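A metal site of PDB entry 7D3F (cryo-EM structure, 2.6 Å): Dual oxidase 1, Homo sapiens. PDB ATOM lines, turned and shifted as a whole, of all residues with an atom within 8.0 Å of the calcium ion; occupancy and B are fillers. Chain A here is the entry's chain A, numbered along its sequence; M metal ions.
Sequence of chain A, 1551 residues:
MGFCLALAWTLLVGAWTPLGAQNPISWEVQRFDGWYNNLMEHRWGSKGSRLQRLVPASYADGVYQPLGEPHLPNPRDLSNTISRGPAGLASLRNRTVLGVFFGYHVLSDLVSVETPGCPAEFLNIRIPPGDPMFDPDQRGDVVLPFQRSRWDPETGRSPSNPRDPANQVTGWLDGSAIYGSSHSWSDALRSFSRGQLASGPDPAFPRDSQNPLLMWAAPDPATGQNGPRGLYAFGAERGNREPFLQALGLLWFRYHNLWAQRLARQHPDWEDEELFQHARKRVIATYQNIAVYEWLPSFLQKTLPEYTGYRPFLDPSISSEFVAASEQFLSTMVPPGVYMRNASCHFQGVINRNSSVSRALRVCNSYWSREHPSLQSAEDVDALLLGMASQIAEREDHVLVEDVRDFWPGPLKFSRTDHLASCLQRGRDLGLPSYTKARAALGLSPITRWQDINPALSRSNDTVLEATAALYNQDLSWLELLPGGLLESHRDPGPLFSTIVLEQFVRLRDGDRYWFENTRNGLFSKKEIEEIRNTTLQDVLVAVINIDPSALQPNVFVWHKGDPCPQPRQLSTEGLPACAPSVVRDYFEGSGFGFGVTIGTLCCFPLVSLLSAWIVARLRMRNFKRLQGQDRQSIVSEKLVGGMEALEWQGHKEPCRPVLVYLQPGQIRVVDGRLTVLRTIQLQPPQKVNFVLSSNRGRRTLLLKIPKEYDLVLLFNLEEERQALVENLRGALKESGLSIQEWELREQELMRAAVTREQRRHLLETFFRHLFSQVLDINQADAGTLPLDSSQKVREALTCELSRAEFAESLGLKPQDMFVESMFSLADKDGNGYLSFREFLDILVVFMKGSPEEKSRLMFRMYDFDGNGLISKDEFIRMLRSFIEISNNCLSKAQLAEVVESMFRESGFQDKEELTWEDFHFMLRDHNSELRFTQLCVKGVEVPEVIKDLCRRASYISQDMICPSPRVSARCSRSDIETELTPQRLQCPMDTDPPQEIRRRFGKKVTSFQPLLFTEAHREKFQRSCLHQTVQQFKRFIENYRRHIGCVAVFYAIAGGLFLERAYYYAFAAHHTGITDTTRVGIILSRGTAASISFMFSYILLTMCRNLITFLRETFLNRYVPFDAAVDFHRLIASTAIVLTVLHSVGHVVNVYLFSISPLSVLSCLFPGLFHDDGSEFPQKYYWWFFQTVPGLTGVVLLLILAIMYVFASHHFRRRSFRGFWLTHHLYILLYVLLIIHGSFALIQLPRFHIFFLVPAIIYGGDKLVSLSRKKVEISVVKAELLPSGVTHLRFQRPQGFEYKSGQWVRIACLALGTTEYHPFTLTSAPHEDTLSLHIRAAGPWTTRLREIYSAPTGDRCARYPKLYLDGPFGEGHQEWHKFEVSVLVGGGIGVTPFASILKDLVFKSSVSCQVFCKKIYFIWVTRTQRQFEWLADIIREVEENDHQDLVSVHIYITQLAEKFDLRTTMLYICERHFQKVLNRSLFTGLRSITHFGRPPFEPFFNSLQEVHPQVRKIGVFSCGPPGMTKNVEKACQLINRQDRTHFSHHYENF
Asp 828 touches the calcium ion (OD1 to CA, 3.5 Å).
Within 4 Å of the calcium ion: Asp 828, Asp 830, Asn 832, Tyr 834 and Glu 839.
The calcium ion is bound by the side-chain carboxylate of Glu 839 (2.5 Å), the side-chain amide oxygen of Asn 832 (2.5 Å), the backbone carbonyl oxygen of Tyr 834 (2.7 Å) and the side-chain carboxylate of Asp 830 (2.8 Å).
Slightly farther from the calcium ion lies OD2 of Asp 830 (2.9 Å).
Slightly farther from the calcium ion lies the side-chain amide nitrogen (ND2) of Asn 832 (3.1 Å).
The side-chain carboxylate (OD2) of Asp 828 sits at hydrogen-bond distance from the backbone NH (N) of Gly 833, 3.1 Å away.
OE1 of Glu 839 is in hydrogen-bond range of N of Lys 829 (3.4 Å).
OE2 of Glu 839 lies close to OG of Ser 836.
The backbone NH of Gly 831 sits at hydrogen-bond distance from the side-chain carboxylate of Asp 828, 3.5 Å away.
The backbone NH (N) of Asn 832 is in hydrogen-bond range of the side-chain carboxylate (OD2) of Asp 828 (3.3 Å).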
ATOM      1  N   GLU A 801      10.625 -19.845 -10.825  1.00  0.00           N
ATOM      2  CA  GLU A 801      10.997 -19.574 -12.201  1.00  0.00           C
ATOM      3  C   GLU A 801      12.142 -18.571 -12.226  1.00  0.00           C
ATOM      4  O   GLU A 801      12.080 -17.532 -11.556  1.00  0.00           O
ATOM      5  CB  GLU A 801       9.799 -19.025 -12.991  1.00  0.00           C
ATOM      6  N   LEU A 802      13.181 -18.883 -12.988  1.00  0.00           N
ATOM      7  CA  LEU A 802      14.372 -18.034 -13.063  1.00  0.00           C
ATOM      8  C   LEU A 802      14.170 -16.939 -14.103  1.00  0.00           C
ATOM      9  O   LEU A 802      13.787 -17.221 -15.249  1.00  0.00           O
ATOM     10  CB  LEU A 802      15.603 -18.865 -13.416  1.00  0.00           C
ATOM     11  CG  LEU A 802      16.376 -19.523 -12.273  1.00  0.00           C
ATOM     12  CD1 LEU A 802      15.531 -20.561 -11.537  1.00  0.00           C
ATOM     13  CD2 LEU A 802      17.641 -20.162 -12.812  1.00  0.00           C
ATOM     14  N   PHE A 824      18.160 -18.684 -23.361  1.00  0.00           N
ATOM     15  CA  PHE A 824      16.953 -18.360 -22.612  1.00  0.00           C
ATOM     16  C   PHE A 824      15.721 -18.395 -23.515  1.00  0.00           C
ATOM     17  O   PHE A 824      14.676 -18.940 -23.116  1.00  0.00           O
ATOM     18  CB  PHE A 824      17.107 -16.991 -21.954  1.00  0.00           C
ATOM     19  CG  PHE A 824      15.907 -16.573 -21.155  1.00  0.00           C
ATOM     20  CD1 PHE A 824      15.660 -17.133 -19.914  1.00  0.00           C
ATOM     21  CD2 PHE A 824      15.042 -15.603 -21.631  1.00  0.00           C
ATOM     22  CE1 PHE A 824      14.572 -16.743 -19.163  1.00  0.00           C
ATOM     23  CE2 PHE A 824      13.940 -15.219 -20.888  1.00  0.00           C
ATOM     24  CZ  PHE A 824      13.710 -15.786 -19.660  1.00  0.00           C
ATOM     25  N   ALA A 827      15.114 -22.116 -24.519  1.00  0.00           N
ATOM     26  CA  ALA A 827      14.656 -22.950 -23.418  1.00  0.00           C
ATOM     27  C   ALA A 827      13.289 -22.541 -22.895  1.00  0.00           C
ATOM     28  O   ALA A 827      12.639 -23.330 -22.199  1.00  0.00           O
ATOM     29  CB  ALA A 827      15.670 -22.918 -22.277  1.00  0.00           C
ATOM     30  N   ASP A 828      12.833 -21.330 -23.203  1.00  0.00           N
ATOM     31  CA  ASP A 828      11.536 -20.851 -22.721  1.00  0.00           C
ATOM     32  C   ASP A 828      10.450 -21.398 -23.643  1.00  0.00           C
ATOM     33  O   ASP A 828      10.124 -20.808 -24.667  1.00  0.00           O
ATOM     34  CB  ASP A 828      11.515 -19.324 -22.661  1.00  0.00           C
ATOM     35  CG  ASP A 828      10.515 -18.804 -21.640  1.00  0.00           C
ATOM     36  OD1 ASP A 828       9.910 -19.627 -20.921  1.00  0.00           O
ATOM     37  OD2 ASP A 828      10.348 -17.565 -21.549  1.00  0.00           O
ATOM     38  N   LYS A 829       9.912 -22.553 -23.263  1.00  0.00           N
ATOM     39  CA  LYS A 829       8.892 -23.202 -24.095  1.00  0.00           C
ATOM     40  C   LYS A 829       7.623 -22.357 -24.182  1.00  0.00           C
ATOM     41  O   LYS A 829       7.095 -22.115 -25.268  1.00  0.00           O
ATOM     42  CB  LYS A 829       8.581 -24.593 -23.542  1.00  0.00           C
ATOM     43  CG  LYS A 829       9.745 -25.569 -23.632  1.00  0.00           C
ATOM     44  CD  LYS A 829       9.451 -26.852 -22.878  1.00  0.00           C
ATOM     45  CE  LYS A 829      10.502 -27.915 -23.143  1.00  0.00           C
ATOM     46  NZ  LYS A 829      11.878 -27.418 -22.877  1.00  0.00           N
ATOM     47  N   ASP A 830       7.116 -21.898 -23.029  1.00  0.00           N
ATOM     48  CA  ASP A 830       5.903 -21.098 -23.014  1.00  0.00           C
ATOM     49  C   ASP A 830       6.162 -19.627 -23.335  1.00  0.00           C
ATOM     50  O   ASP A 830       5.208 -18.906 -23.647  1.00  0.00           O
ATOM     51  CB  ASP A 830       5.202 -21.220 -21.664  1.00  0.00           C
ATOM     52  CG  ASP A 830       6.126 -20.894 -20.505  1.00  0.00           C
ATOM     53  OD1 ASP A 830       7.354 -20.968 -20.677  1.00  0.00           O
ATOM     54  OD2 ASP A 830       5.609 -20.561 -19.413  1.00  0.00           O
ATOM     55  N   GLY A 831       7.411 -19.182 -23.272  1.00  0.00           N
ATOM     56  CA  GLY A 831       7.732 -17.806 -23.604  1.00  0.00           C
ATOM     57  C   GLY A 831       7.088 -16.775 -22.697  1.00  0.00           C
ATOM     58  O   GLY A 831       6.607 -15.742 -23.174  1.00  0.00           O
ATOM     59  N   ASN A 832       7.082 -17.032 -21.391  1.00  0.00           N
ATOM     60  CA  ASN A 832       6.494 -16.123 -20.413  1.00  0.00           C
ATOM     61  C   ASN A 832       7.505 -15.155 -19.830  1.00  0.00           C
ATOM     62  O   ASN A 832       7.159 -14.380 -18.923  1.00  0.00           O
ATOM     63  CB  ASN A 832       5.819 -16.916 -19.287  1.00  0.00           C
ATOM     64  CG  ASN A 832       6.785 -17.856 -18.584  1.00  0.00           C
ATOM     65  OD1 ASN A 832       7.676 -18.418 -19.213  1.00  0.00           O
ATOM     66  ND2 ASN A 832       6.592 -18.031 -17.288  1.00  0.00           N
ATOM     67  N   GLY A 833       8.742 -15.172 -20.317  1.00  0.00           N
ATOM     68  CA  GLY A 833       9.789 -14.323 -19.791  1.00  0.00           C
ATOM     69  C   GLY A 833      10.519 -14.880 -18.589  1.00  0.00           C
ATOM     70  O   GLY A 833      11.469 -14.233 -18.110  1.00  0.00           O
ATOM     71  N   TYR A 834      10.116 -16.043 -18.089  1.00  0.00           N
ATOM     72  CA  TYR A 834      10.779 -16.696 -16.969  1.00  0.00           C
ATOM     73  C   TYR A 834      10.990 -18.160 -17.302  1.00  0.00           C
ATOM     74  O   TYR A 834      10.203 -18.776 -18.021  1.00  0.00           O
ATOM     75  CB  TYR A 834       9.955 -16.559 -15.666  1.00  0.00           C
ATOM     76  CG  TYR A 834       9.889 -15.144 -15.134  1.00  0.00           C
ATOM     77  CD1 TYR A 834       9.022 -14.209 -15.680  1.00  0.00           C
ATOM     78  CD2 TYR A 834      10.683 -14.748 -14.064  1.00  0.00           C
ATOM     79  CE1 TYR A 834       8.950 -12.920 -15.189  1.00  0.00           C
ATOM     80  CE2 TYR A 834      10.612 -13.459 -13.562  1.00  0.00           C
ATOM     81  CZ  TYR A 834       9.754 -12.549 -14.131  1.00  0.00           C
ATOM     82  OH  TYR A 834       9.679 -11.270 -13.639  1.00  0.00           O
ATOM     83  N   LEU A 835      12.063 -18.732 -16.765  1.00  0.00           N
ATOM     84  CA  LEU A 835      12.461 -20.108 -17.048  1.00  0.00           C
ATOM     85  C   LEU A 835      12.169 -20.959 -15.813  1.00  0.00           C
ATOM     86  O   LEU A 835      12.680 -20.680 -14.729  1.00  0.00           O
ATOM     87  CB  LEU A 835      13.930 -20.186 -17.432  1.00  0.00           C
ATOM     88  CG  LEU A 835      14.350 -21.254 -18.455  1.00  0.00           C
ATOM     89  CD1 LEU A 835      15.700 -20.912 -19.048  1.00  0.00           C
ATOM     90  CD2 LEU A 835      14.379 -22.626 -17.826  1.00  0.00           C
ATOM     91  N   SER A 836      11.370 -22.010 -15.987  1.00  0.00           N
ATOM     92  CA  SER A 836      10.939 -22.854 -14.891  1.00  0.00           C
ATOM     93  C   SER A 836      11.847 -24.085 -14.780  1.00  0.00           C
ATOM     94  O   SER A 836      12.764 -24.295 -15.581  1.00  0.00           O
ATOM     95  CB  SER A 836       9.478 -23.266 -15.071  1.00  0.00           C
ATOM     96  OG  SER A 836       9.313 -24.022 -16.258  1.00  0.00           O
ATOM     97  N   PHE A 837      11.579 -24.912 -13.771  1.00  0.00           N
ATOM     98  CA  PHE A 837      12.377 -26.112 -13.550  1.00  0.00           C
ATOM     99  C   PHE A 837      12.214 -27.109 -14.690  1.00  0.00           C
ATOM    100  O   PHE A 837      13.190 -27.744 -15.110  1.00  0.00           O
ATOM    101  CB  PHE A 837      11.997 -26.762 -12.218  1.00  0.00           C
ATOM    102  CG  PHE A 837      12.831 -27.958 -11.861  1.00  0.00           C
ATOM    103  CD1 PHE A 837      13.991 -27.811 -11.097  1.00  0.00           C
ATOM    104  CD2 PHE A 837      12.463 -29.235 -12.260  1.00  0.00           C
ATOM    105  CE1 PHE A 837      14.757 -28.912 -10.759  1.00  0.00           C
ATOM    106  CE2 PHE A 837      13.238 -30.339 -11.923  1.00  0.00           C
ATOM    107  CZ  PHE A 837      14.383 -30.167 -11.177  1.00  0.00           C
ATOM    108  N   ARG A 838      10.992 -27.278 -15.200  1.00  0.00           N
ATOM    109  CA  ARG A 838      10.724 -28.308 -16.201  1.00  0.00           C
ATOM    110  C   ARG A 838      11.498 -28.028 -17.490  1.00  0.00           C
ATOM    111  O   ARG A 838      12.126 -28.933 -18.049  1.00  0.00           O
ATOM    112  CB  ARG A 838       9.228 -28.397 -16.472  1.00  0.00           C
ATOM    113  CG  ARG A 838       8.814 -29.602 -17.289  1.00  0.00           C
ATOM    114  CD  ARG A 838       9.166 -30.888 -16.560  1.00  0.00           C
ATOM    115  NE  ARG A 838      10.079 -31.727 -17.337  1.00  0.00           N
ATOM    116  CZ  ARG A 838      10.680 -32.810 -16.869  1.00  0.00           C
ATOM    117  NH1 ARG A 838      10.473 -33.194 -15.613  1.00  0.00           N
ATOM    118  NH2 ARG A 838      11.490 -33.510 -17.638  1.00  0.00           N
ATOM    119  N   GLU A 839      11.434 -26.796 -17.984  1.00  0.00           N
ATOM    120  CA  GLU A 839      12.120 -26.454 -19.228  1.00  0.00           C
ATOM    121  C   GLU A 839      13.631 -26.607 -19.083  1.00  0.00           C
ATOM    122  O   GLU A 839      14.288 -27.126 -19.987  1.00  0.00           O
ATOM    123  CB  GLU A 839      11.768 -25.017 -19.621  1.00  0.00           C
ATOM    124  CG  GLU A 839      10.317 -24.656 -19.379  1.00  0.00           C
ATOM    125  CD  GLU A 839      10.089 -23.155 -19.285  1.00  0.00           C
ATOM    126  OE1 GLU A 839      10.818 -22.402 -19.954  1.00  0.00           O
ATOM    127  OE2 GLU A 839       9.193 -22.743 -18.515  1.00  0.00           O
HETATM  128 CA    CA M   1       8.218 -20.537 -18.048  1.00  0.00          CA
